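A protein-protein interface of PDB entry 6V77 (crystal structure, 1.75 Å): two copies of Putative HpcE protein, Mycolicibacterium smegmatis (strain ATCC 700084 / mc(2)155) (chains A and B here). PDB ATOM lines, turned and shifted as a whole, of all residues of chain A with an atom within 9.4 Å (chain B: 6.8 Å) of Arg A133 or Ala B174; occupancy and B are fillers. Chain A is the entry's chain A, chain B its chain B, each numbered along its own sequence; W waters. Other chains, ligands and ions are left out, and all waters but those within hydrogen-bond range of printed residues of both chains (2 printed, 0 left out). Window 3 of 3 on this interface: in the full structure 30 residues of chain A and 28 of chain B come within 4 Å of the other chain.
OE1 of Gln A71 sits at hydrogen-bond distance from OG of Ser B102.
The backbone NH of Glu A230 lies within hydrogen-bond range of the side-chain hydroxyl of Ser B102 (3.4 Å).
NE2 of Gln A71 is in hydrogen-bond range of O of Glu A230, 2.8 Å away.
NH1 of Arg A133 sits at hydrogen-bond distance from O of Thr A228 (2.9 Å).
Ser B102 touches Arg A133 (O to NH2, 3.7 Å).
Ala B174 touches Arg A133 (CB to NH2, 3.6 Å).
Ser B172 touches Thr A228.
His B173 touches Thr A228 (CA to O, 3.6 Å).
Thr A228 touches Ala B174.
Val A229 touches Ser B102 (CB to OG, 3.5 Å).
CG1 of Val A229 touches O of Ser B172 (3.7 Å).
Ser B102 touches Tyr A232 (CA to OH, 3.3 Å).
Of the printed residues of chain B, Gln A71 touches Ser B102 (2.6 Å).
Arg A133 touches two residues of chain B.
Printed residues of chain B within 4 Å of Glu A230: Ser B102.
Of the printed residues of chain A, His B173 touches Thr A228 (3.6 Å).
Ala B174 touches just these residues of chain A: Arg A133 (3.6 Å) and Thr A228 (3.9 Å).
The nearest residue of chain A that does not touch Ala B174 is Val A229 (5.9 Å).
The nearest printed residue of chain B that does not touch Gln A71 is Ser B103 (5.0 Å).
Hydrophobic or aromatic side chains of chain A within 4 Å of the printed part of chain B: Val A229 and Tyr A232.
Of the 14 printed residues of chain B, 4 touch a printed residue of chain A.
No position is printed for both chains.
Water W2 lies within hydrogen-bond range of the backbone carbonyl oxygen (O) of Ser B172 (2.7 Å), the guanidinium group (NH2) of Arg A133 (2.9 Å) and the side-chain hydroxyl (OG) of Ser B102 (3.0 Å).
Water W1 lies within hydrogen-bond range of the side-chain carboxylate of Glu A230 (2.7 Å), the guanidinium group of Arg A133 (2.8 Å) and the backbone carbonyl oxygen of Ser B102 (3.5 Å).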
ATOM      1  N   GLN A  71      10.989  -0.853  14.839  1.00  0.00           N
ATOM      2  CA  GLN A  71      10.328  -0.028  15.840  1.00  0.00           C
ATOM      3  C   GLN A  71       9.562  -0.937  16.798  1.00  0.00           C
ATOM      4  O   GLN A  71       8.888  -1.881  16.364  1.00  0.00           O
ATOM      5  CB  GLN A  71       9.344   0.991  15.177  1.00  0.00           C
ATOM      6  CG  GLN A  71      10.053   1.939  14.201  1.00  0.00           C
ATOM      7  CD  GLN A  71       9.116   2.877  13.441  1.00  0.00           C
ATOM      8  OE1 GLN A  71       9.390   4.078  13.320  1.00  0.00           O
ATOM      9  NE2 GLN A  71       8.032   2.319  12.881  1.00  0.00           N
ATOM     10  N   MET A 128       3.648  -6.580  12.830  1.00  0.00           N
ATOM     11  CA  MET A 128       3.069  -6.041  11.605  1.00  0.00           C
ATOM     12  C   MET A 128       3.523  -6.844  10.393  1.00  0.00           C
ATOM     13  O   MET A 128       4.680  -7.271  10.310  1.00  0.00           O
ATOM     14  CB  MET A 128       3.472  -4.582  11.420  1.00  0.00           C
ATOM     15  CG  MET A 128       3.099  -3.691  12.600  1.00  0.00           C
ATOM     16  SD  MET A 128       1.310  -3.647  12.887  1.00  0.00           S
ATOM     17  CE  MET A 128       0.706  -3.016  11.323  1.00  0.00           C
ATOM     18  N   ARG A 130       2.324  -5.518   7.265  1.00  0.00           N
ATOM     19  CA  ARG A 130       2.237  -4.455   6.279  1.00  0.00           C
ATOM     20  C   ARG A 130       2.309  -3.139   7.037  1.00  0.00           C
ATOM     21  O   ARG A 130       1.826  -3.045   8.170  1.00  0.00           O
ATOM     22  CB  ARG A 130       0.927  -4.534   5.485  1.00  0.00           C
ATOM     23  CG  ARG A 130       0.870  -3.586   4.316  1.00  0.00           C
ATOM     24  CD  ARG A 130      -0.429  -3.773   3.560  1.00  0.00           C
ATOM     25  NE  ARG A 130      -0.610  -5.172   3.199  1.00  0.00           N
ATOM     26  CZ  ARG A 130      -1.742  -5.678   2.727  1.00  0.00           C
ATOM     27  NH1 ARG A 130      -2.797  -4.891   2.563  1.00  0.00           N
ATOM     28  NH2 ARG A 130      -1.819  -6.968   2.424  1.00  0.00           N
ATOM     29  N   GLY A 131       2.904  -2.125   6.413  1.00  0.00           N
ATOM     30  CA  GLY A 131       3.084  -0.859   7.102  1.00  0.00           C
ATOM     31  C   GLY A 131       2.442   0.328   6.416  1.00  0.00           C
ATOM     32  O   GLY A 131       1.592   0.160   5.534  1.00  0.00           O
ATOM     33  N   GLY A 132       2.836   1.532   6.836  1.00  0.00           N
ATOM     34  CA  GLY A 132       2.320   2.772   6.273  1.00  0.00           C
ATOM     35  C   GLY A 132       2.003   3.812   7.331  1.00  0.00           C
ATOM     36  O   GLY A 132       2.125   3.547   8.525  1.00  0.00           O
ATOM     37  N   ARG A 133       1.616   5.013   6.871  1.00  0.00           N
ATOM     38  CA  ARG A 133       1.033   6.038   7.720  1.00  0.00           C
ATOM     39  C   ARG A 133      -0.473   6.088   7.485  1.00  0.00           C
ATOM     40  O   ARG A 133      -0.967   5.702   6.426  1.00  0.00           O
ATOM     41  CB  ARG A 133       1.661   7.411   7.421  1.00  0.00           C
ATOM     42  CG  ARG A 133       3.180   7.477   7.700  1.00  0.00           C
ATOM     43  CD  ARG A 133       3.766   8.868   7.369  1.00  0.00           C
ATOM     44  NE  ARG A 133       5.207   8.889   7.626  1.00  0.00           N
ATOM     45  CZ  ARG A 133       5.740   9.150   8.816  1.00  0.00           C
ATOM     46  NH1 ARG A 133       4.947   9.442   9.845  1.00  0.00           N
ATOM     47  NH2 ARG A 133       7.064   9.109   8.981  1.00  0.00           N
ATOM     48  N   ASN A 134      -1.196   6.575   8.489  1.00  0.00           N
ATOM     49  CA  ASN A 134      -2.656   6.697   8.428  1.00  0.00           C
ATOM     50  C   ASN A 134      -3.314   5.386   7.977  1.00  0.00           C
ATOM     51  O   ASN A 134      -4.133   5.348   7.051  1.00  0.00           O
ATOM     52  CB  ASN A 134      -3.061   7.858   7.524  1.00  0.00           C
ATOM     53  CG  ASN A 134      -2.515   9.192   8.006  1.00  0.00           C
ATOM     54  OD1 ASN A 134      -1.936   9.957   7.229  1.00  0.00           O
ATOM     55  ND2 ASN A 134      -2.721   9.488   9.285  1.00  0.00           N
ATOM     56  N   ILE A 135      -2.958   4.308   8.656  1.00  0.00           N
ATOM     57  CA  ILE A 135      -3.605   3.012   8.399  1.00  0.00           C
ATOM     58  C   ILE A 135      -5.045   3.077   8.894  1.00  0.00           C
ATOM     59  O   ILE A 135      -5.278   3.435  10.062  1.00  0.00           O
ATOM     60  CB  ILE A 135      -2.839   1.896   9.090  1.00  0.00           C
ATOM     61  CG1 ILE A 135      -1.415   1.796   8.521  1.00  0.00           C
ATOM     62  CG2 ILE A 135      -3.599   0.582   8.920  1.00  0.00           C
ATOM     63  CD1 ILE A 135      -0.455   0.876   9.315  1.00  0.00           C
ATOM     64  N   PRO A 136      -6.035   2.762   8.058  1.00  0.00           N
ATOM     65  CA  PRO A 136      -7.441   2.885   8.487  1.00  0.00           C
ATOM     66  C   PRO A 136      -7.768   1.848   9.561  1.00  0.00           C
ATOM     67  O   PRO A 136      -7.402   0.678   9.454  1.00  0.00           O
ATOM     68  CB  PRO A 136      -8.228   2.636   7.195  1.00  0.00           C
ATOM     69  CG  PRO A 136      -7.325   1.775   6.369  1.00  0.00           C
ATOM     70  CD  PRO A 136      -5.916   2.264   6.676  1.00  0.00           C
ATOM     71  N   GLU A 137      -8.430   2.305  10.622  1.00  0.00           N
ATOM     72  CA  GLU A 137      -8.720   1.422  11.746  1.00  0.00           C
ATOM     73  C   GLU A 137      -9.574   0.232  11.314  1.00  0.00           C
ATOM     74  O   GLU A 137      -9.377  -0.892  11.792  1.00  0.00           O
ATOM     75  CB  GLU A 137      -9.410   2.224  12.845  1.00  0.00           C
ATOM     76  CG  GLU A 137      -9.772   1.464  14.083  1.00  0.00           C
ATOM     77  CD  GLU A 137     -10.085   2.404  15.235  1.00  0.00           C
ATOM     78  OE1 GLU A 137     -10.581   1.932  16.276  1.00  0.00           O
ATOM     79  OE2 GLU A 137      -9.825   3.621  15.100  1.00  0.00           O
ATOM     80  N   PHE A 143      -3.239  -5.602   8.220  1.00  0.00           N
ATOM     81  CA  PHE A 143      -1.830  -5.224   8.257  1.00  0.00           C
ATOM     82  C   PHE A 143      -1.026  -6.022   9.277  1.00  0.00           C
ATOM     83  O   PHE A 143       0.181  -5.792   9.411  1.00  0.00           O
ATOM     84  CB  PHE A 143      -1.679  -3.719   8.556  1.00  0.00           C
ATOM     85  CG  PHE A 143      -2.189  -2.829   7.453  1.00  0.00           C
ATOM     86  CD1 PHE A 143      -3.538  -2.802   7.132  1.00  0.00           C
ATOM     87  CD2 PHE A 143      -1.314  -2.014   6.741  1.00  0.00           C
ATOM     88  CE1 PHE A 143      -4.015  -1.967   6.112  1.00  0.00           C
ATOM     89  CE2 PHE A 143      -1.789  -1.165   5.724  1.00  0.00           C
ATOM     90  CZ  PHE A 143      -3.136  -1.163   5.406  1.00  0.00           C
ATOM     91  N   ILE A 222      -3.004   0.371  16.121  1.00  0.00           N
ATOM     92  CA  ILE A 222      -2.306   0.437  14.841  1.00  0.00           C
ATOM     93  C   ILE A 222      -2.623   1.747  14.138  1.00  0.00           C
ATOM     94  O   ILE A 222      -1.720   2.464  13.681  1.00  0.00           O
ATOM     95  CB  ILE A 222      -2.688  -0.767  13.967  1.00  0.00           C
ATOM     96  CG1 ILE A 222      -2.041  -2.034  14.538  1.00  0.00           C
ATOM     97  CG2 ILE A 222      -2.291  -0.533  12.522  1.00  0.00           C
ATOM     98  CD1 ILE A 222      -2.603  -3.296  13.950  1.00  0.00           C
ATOM     99  N   ALA A 223      -3.914   2.069  14.025  1.00  0.00           N
ATOM    100  CA  ALA A 223      -4.319   3.307  13.365  1.00  0.00           C
ATOM    101  C   ALA A 223      -3.695   4.520  14.043  1.00  0.00           C
ATOM    102  O   ALA A 223      -3.101   5.384  13.381  1.00  0.00           O
ATOM    103  CB  ALA A 223      -5.851   3.413  13.362  1.00  0.00           C
ATOM    104  N   TYR A 224      -3.798   4.578  15.374  1.00  0.00           N
ATOM    105  CA  TYR A 224      -3.309   5.729  16.128  1.00  0.00           C
ATOM    106  C   TYR A 224      -1.802   5.900  15.972  1.00  0.00           C
ATOM    107  O   TYR A 224      -1.311   7.007  15.713  1.00  0.00           O
ATOM    108  CB  TYR A 224      -3.672   5.579  17.605  1.00  0.00           C
ATOM    109  CG  TYR A 224      -3.090   6.707  18.418  1.00  0.00           C
ATOM    110  CD1 TYR A 224      -3.681   7.972  18.418  1.00  0.00           C
ATOM    111  CD2 TYR A 224      -1.927   6.522  19.153  1.00  0.00           C
ATOM    112  CE1 TYR A 224      -3.127   9.027  19.146  1.00  0.00           C
ATOM    113  CE2 TYR A 224      -1.370   7.569  19.880  1.00  0.00           C
ATOM    114  CZ  TYR A 224      -1.965   8.805  19.870  1.00  0.00           C
ATOM    115  OH  TYR A 224      -1.395   9.823  20.601  1.00  0.00           O
ATOM    116  N   LEU A 225      -1.044   4.813  16.137  1.00  0.00           N
ATOM    117  CA  LEU A 225       0.399   4.916  15.962  1.00  0.00           C
ATOM    118  C   LEU A 225       0.728   5.454  14.580  1.00  0.00           C
ATOM    119  O   LEU A 225       1.553   6.359  14.429  1.00  0.00           O
ATOM    120  CB  LEU A 225       1.054   3.547  16.174  1.00  0.00           C
ATOM    121  CG  LEU A 225       1.044   3.084  17.633  1.00  0.00           C
ATOM    122  CD1 LEU A 225       1.477   1.614  17.740  1.00  0.00           C
ATOM    123  CD2 LEU A 225       1.965   3.986  18.466  1.00  0.00           C
ATOM    124  N   SER A 226       0.076   4.900  13.553  1.00  0.00           N
ATOM    125  CA  SER A 226       0.346   5.268  12.172  1.00  0.00           C
ATOM    126  C   SER A 226      -0.050   6.706  11.853  1.00  0.00           C
ATOM    127  O   SER A 226       0.326   7.208  10.787  1.00  0.00           O
ATOM    128  CB  SER A 226      -0.394   4.312  11.233  1.00  0.00           C
ATOM    129  OG  SER A 226      -1.757   4.704  11.091  1.00  0.00           O
ATOM    130  N   ASP A 227      -0.797   7.380  12.736  1.00  0.00           N
ATOM    131  CA  ASP A 227      -1.106   8.789  12.515  1.00  0.00           C
ATOM    132  C   ASP A 227       0.053   9.712  12.895  1.00  0.00           C
ATOM    133  O   ASP A 227      -0.006  10.910  12.584  1.00  0.00           O
ATOM    134  CB  ASP A 227      -2.371   9.178  13.289  1.00  0.00           C
ATOM    135  CG  ASP A 227      -3.635   8.527  12.725  1.00  0.00           C
ATOM    136  OD1 ASP A 227      -3.586   7.992  11.598  1.00  0.00           O
ATOM    137  OD2 ASP A 227      -4.684   8.558  13.408  1.00  0.00           O
ATOM    138  N   THR A 228       1.113   9.176  13.527  1.00  0.00           N
ATOM    139  CA  THR A 228       2.329   9.926  13.833  1.00  0.00           C
ATOM    140  C   THR A 228       3.581   9.333  13.197  1.00  0.00           C
ATOM    141  O   THR A 228       4.396  10.091  12.638  1.00  0.00           O
ATOM    142  CB  THR A 228       2.510  10.040  15.367  1.00  0.00           C
ATOM    143  OG1 THR A 228       1.432  10.823  15.919  1.00  0.00           O
ATOM    144  CG2 THR A 228       3.836  10.745  15.703  1.00  0.00           C
ATOM    145  N   VAL A 229       3.756   8.011  13.260  1.00  0.00           N
ATOM    146  CA  VAL A 229       4.920   7.336  12.697  1.00  0.00           C
ATOM    147  C   VAL A 229       4.506   6.568  11.445  1.00  0.00           C
ATOM    148  O   VAL A 229       3.325   6.337  11.188  1.00  0.00           O
ATOM    149  CB  VAL A 229       5.594   6.383  13.709  1.00  0.00           C
ATOM    150  CG1 VAL A 229       6.037   7.135  14.943  1.00  0.00           C
ATOM    151  CG2 VAL A 229       4.670   5.204  14.078  1.00  0.00           C
ATOM    152  N   GLU A 230       5.507   6.147  10.671  1.00  0.00           N
ATOM    153  CA  GLU A 230       5.286   5.146   9.636  1.00  0.00           C
ATOM    154  C   GLU A 230       5.530   3.780  10.265  1.00  0.00           C
ATOM    155  O   GLU A 230       6.633   3.524  10.742  1.00  0.00           O
ATOM    156  CB  GLU A 230       6.233   5.365   8.456  1.00  0.00           C
ATOM    157  CG  GLU A 230       6.014   4.316   7.353  1.00  0.00           C
ATOM    158  CD  GLU A 230       6.943   4.480   6.174  1.00  0.00           C
ATOM    159  OE1 GLU A 230       7.778   5.401   6.194  1.00  0.00           O
ATOM    160  OE2 GLU A 230       6.848   3.671   5.233  1.00  0.00           O
ATOM    161  N   LEU A 231       4.513   2.919  10.295  1.00  0.00           N
ATOM    162  CA  LEU A 231       4.759   1.549  10.744  1.00  0.00           C
ATOM    163  C   LEU A 231       5.434   0.761   9.628  1.00  0.00           C
ATOM    164  O   LEU A 231       5.209   1.015   8.443  1.00  0.00           O
ATOM    165  CB  LEU A 231       3.456   0.865  11.159  1.00  0.00           C
ATOM    166  CG  LEU A 231       2.746   1.507  12.354  1.00  0.00           C
ATOM    167  CD1 LEU A 231       1.452   0.756  12.628  1.00  0.00           C
ATOM    168  CD2 LEU A 231       3.655   1.472  13.577  1.00  0.00           C
ATOM    169  N   TYR A 232       6.271  -0.206  10.019  1.00  0.00           N
ATOM    170  CA  TYR A 232       6.983  -1.058   9.082  1.00  0.00           C
ATOM    171  C   TYR A 232       6.583  -2.513   9.269  1.00  0.00           C
ATOM    172  O   TYR A 232       6.290  -2.930  10.390  1.00  0.00           O
ATOM    173  CB  TYR A 232       8.491  -0.991   9.296  1.00  0.00           C
ATOM    174  CG  TYR A 232       9.102   0.359   9.094  1.00  0.00           C
ATOM    175  CD1 TYR A 232       9.057   0.971   7.856  1.00  0.00           C
ATOM    176  CD2 TYR A 232       9.759   1.009  10.140  1.00  0.00           C
ATOM    177  CE1 TYR A 232       9.638   2.217   7.653  1.00  0.00           C
ATOM    178  CE2 TYR A 232      10.344   2.271   9.939  1.00  0.00           C
ATOM    179  CZ  TYR A 232      10.280   2.846   8.692  1.00  0.00           C
ATOM    180  OH  TYR A 232      10.865   4.066   8.476  1.00  0.00           O
ATOM    181  N   SER B 102      11.460   5.757  12.019  1.00  0.00           N
ATOM    182  CA  SER B 102      10.773   6.296  10.852  1.00  0.00           C
ATOM    183  C   SER B 102      10.830   7.823  10.791  1.00  0.00           C
ATOM    184  O   SER B 102      10.570   8.373   9.723  1.00  0.00           O
ATOM    185  CB  SER B 102       9.297   5.868  10.800  1.00  0.00           C
ATOM    186  OG  SER B 102       8.607   6.220  11.985  1.00  0.00           O
ATOM    187  N   SER B 103      11.158   8.498  11.901  1.00  0.00           N
ATOM    188  CA  SER B 103      11.270   9.956  11.943  1.00  0.00           C
ATOM    189  C   SER B 103      12.662  10.458  11.604  1.00  0.00           C
ATOM    190  O   SER B 103      12.858  11.675  11.503  1.00  0.00           O
ATOM    191  CB  SER B 103      10.896  10.486  13.334  1.00  0.00           C
ATOM    192  OG  SER B 103      11.883  10.120  14.289  1.00  0.00           O
ATOM    193  N   ILE B 104      13.640   9.571  11.461  1.00  0.00           N
ATOM    194  CA  ILE B 104      15.011  10.004  11.223  1.00  0.00           C
ATOM    195  C   ILE B 104      15.167  10.350   9.751  1.00  0.00           C
ATOM    196  O   ILE B 104      14.749   9.588   8.870  1.00  0.00           O
ATOM    197  CB  ILE B 104      16.008   8.916  11.659  1.00  0.00           C
ATOM    198  CG1 ILE B 104      16.055   8.851  13.187  1.00  0.00           C
ATOM    199  CG2 ILE B 104      17.415   9.190  11.060  1.00  0.00           C
ATOM    200  CD1 ILE B 104      16.965   7.755  13.739  1.00  0.00           C
ATOM    201  N   THR B 105      15.750  11.512   9.484  1.00  0.00           N
ATOM    202  CA  THR B 105      16.070  11.938   8.132  1.00  0.00           C
ATOM    203  C   THR B 105      17.450  12.576   8.155  1.00  0.00           C
ATOM    204  O   THR B 105      18.058  12.755   9.213  1.00  0.00           O
ATOM    205  CB  THR B 105      15.060  12.959   7.603  1.00  0.00           C
ATOM    206  OG1 THR B 105      15.208  14.154   8.365  1.00  0.00           O
ATOM    207  CG2 THR B 105      13.613  12.440   7.744  1.00  0.00           C
ATOM    208  N   VAL B 111      10.273  20.791   6.566  1.00  0.00           N
ATOM    209  CA  VAL B 111       9.644  19.927   7.560  1.00  0.00           C
ATOM    210  C   VAL B 111       8.179  20.312   7.669  1.00  0.00           C
ATOM    211  O   VAL B 111       7.850  21.500   7.795  1.00  0.00           O
ATOM    212  CB  VAL B 111      10.329  20.033   8.937  1.00  0.00           C
ATOM    213  CG1 VAL B 111       9.625  19.147   9.960  1.00  0.00           C
ATOM    214  CG2 VAL B 111      11.815  19.707   8.834  1.00  0.00           C
ATOM    215  N   GLN B 112       7.303  19.309   7.626  1.00  0.00           N
ATOM    216  CA  GLN B 112       5.873  19.554   7.749  1.00  0.00           C
ATOM    217  C   GLN B 112       5.530  19.766   9.217  1.00  0.00           C
ATOM    218  O   GLN B 112       5.959  18.990  10.079  1.00  0.00           O
ATOM    219  CB  GLN B 112       5.079  18.380   7.165  1.00  0.00           C
ATOM    220  CG  GLN B 112       5.364  18.113   5.683  1.00  0.00           C
ATOM    221  CD  GLN B 112       4.782  19.185   4.765  1.00  0.00           C
ATOM    222  OE1 GLN B 112       3.671  19.672   4.986  1.00  0.00           O
ATOM    223  NE2 GLN B 112       5.529  19.551   3.728  1.00  0.00           N
ATOM    224  N   PRO B 114       2.969  19.398  11.948  1.00  0.00           N
ATOM    225  CA  PRO B 114       1.690  18.867  12.415  1.00  0.00           C
ATOM    226  C   PRO B 114       0.968  19.918  13.235  1.00  0.00           C
ATOM    227  O   PRO B 114       1.563  20.891  13.707  1.00  0.00           O
ATOM    228  CB  PRO B 114       2.098  17.676  13.281  1.00  0.00           C
ATOM    229  CG  PRO B 114       3.463  18.042  13.763  1.00  0.00           C
ATOM    230  CD  PRO B 114       4.113  18.760  12.623  1.00  0.00           C
ATOM    231  N   LEU B 153      12.998  17.744  17.293  1.00  0.00           N
ATOM    232  CA  LEU B 153      11.765  18.506  17.124  1.00  0.00           C
ATOM    233  C   LEU B 153      10.665  17.829  17.925  1.00  0.00           C
ATOM    234  O   LEU B 153      10.588  16.602  17.969  1.00  0.00           O
ATOM    235  CB  LEU B 153      11.383  18.600  15.649  1.00  0.00           C
ATOM    236  CG  LEU B 153      12.434  19.338  14.819  1.00  0.00           C
ATOM    237  CD1 LEU B 153      12.176  19.182  13.330  1.00  0.00           C
ATOM    238  CD2 LEU B 153      12.371  20.813  15.196  1.00  0.00           C
ATOM    239  N   SER B 172       8.482  12.081  17.213  1.00  0.00           N
ATOM    240  CA  SER B 172       8.686  11.100  16.152  1.00  0.00           C
ATOM    241  C   SER B 172       7.762  11.325  14.966  1.00  0.00           C
ATOM    242  O   SER B 172       7.525  10.396  14.187  1.00  0.00           O
ATOM    243  CB  SER B 172       8.508   9.670  16.686  1.00  0.00           C
ATOM    244  OG  SER B 172       9.439   9.435  17.716  1.00  0.00           O
ATOM    245  N   HIS B 173       7.187  12.528  14.832  1.00  0.00           N
ATOM    246  CA  HIS B 173       6.497  12.859  13.602  1.00  0.00           C
ATOM    247  C   HIS B 173       7.463  12.784  12.429  1.00  0.00           C
ATOM    248  O   HIS B 173       8.679  12.797  12.603  1.00  0.00           O
ATOM    249  CB  HIS B 173       5.914  14.272  13.675  1.00  0.00           C
ATOM    250  CG  HIS B 173       4.720  14.382  14.565  1.00  0.00           C
ATOM    251  ND1 HIS B 173       3.429  14.276  14.091  1.00  0.00           N
ATOM    252  CD2 HIS B 173       4.616  14.615  15.895  1.00  0.00           C
ATOM    253  CE1 HIS B 173       2.581  14.437  15.091  1.00  0.00           C
ATOM    254  NE2 HIS B 173       3.274  14.650  16.196  1.00  0.00           N
ATOM    255  N   ALA B 174       6.918  12.723  11.218  1.00  0.00           N
ATOM    256  CA  ALA B 174       7.784  12.676  10.040  1.00  0.00           C
ATOM    257  C   ALA B 174       8.765  13.841  10.045  1.00  0.00           C
ATOM    258  O   ALA B 174       8.366  15.001  10.202  1.00  0.00           O
ATOM    259  CB  ALA B 174       6.944  12.715   8.764  1.00  0.00           C
ATOM    260  N   GLY B 175      10.045  13.521   9.875  1.00  0.00           N
ATOM    261  CA  GLY B 175      11.103  14.503   9.797  1.00  0.00           C
ATOM    262  C   GLY B 175      11.468  15.155  11.105  1.00  0.00           C
ATOM    263  O   GLY B 175      12.234  16.124  11.095  1.00  0.00           O
ATOM    264  N   PHE B 176      10.955  14.659  12.229  1.00  0.00           N
ATOM    265  CA  PHE B 176      11.293  15.264  13.515  1.00  0.00           C
ATOM    266  C   PHE B 176      12.662  14.867  14.064  1.00  0.00           C
ATOM    267  O   PHE B 176      13.039  15.378  15.125  1.00  0.00           O
ATOM    268  CB  PHE B 176      10.208  14.955  14.559  1.00  0.00           C
ATOM    269  CG  PHE B 176       9.067  15.975  14.589  1.00  0.00           C
ATOM    270  CD1 PHE B 176       8.721  16.700  13.447  1.00  0.00           C
ATOM    271  CD2 PHE B 176       8.340  16.195  15.758  1.00  0.00           C
ATOM    272  CE1 PHE B 176       7.668  17.629  13.463  1.00  0.00           C
ATOM    273  CE2 PHE B 176       7.266  17.124  15.785  1.00  0.00           C
ATOM    274  CZ  PHE B 176       6.953  17.852  14.640  1.00  0.00           C
ATOM    275  N   SER B 177      13.432  14.011  13.387  1.00  0.00           N
ATOM    276  CA  SER B 177      14.760  13.610  13.861  1.00  0.00           C
ATOM    277  C   SER B 177      15.802  13.757  12.761  1.00  0.00           C
ATOM    278  O   SER B 177      16.430  12.774  12.350  1.00  0.00           O
ATOM    279  CB  SER B 177      14.728  12.171  14.385  1.00  0.00           C
ATOM    280  OG  SER B 177      13.600  12.012  15.227  1.00  0.00           O
HETATM  281  O   HOH W   1       8.528   7.934   6.934  1.00  0.00           O
HETATM  282  O   HOH W   2       7.661   9.064  11.827  1.00  0.00           O
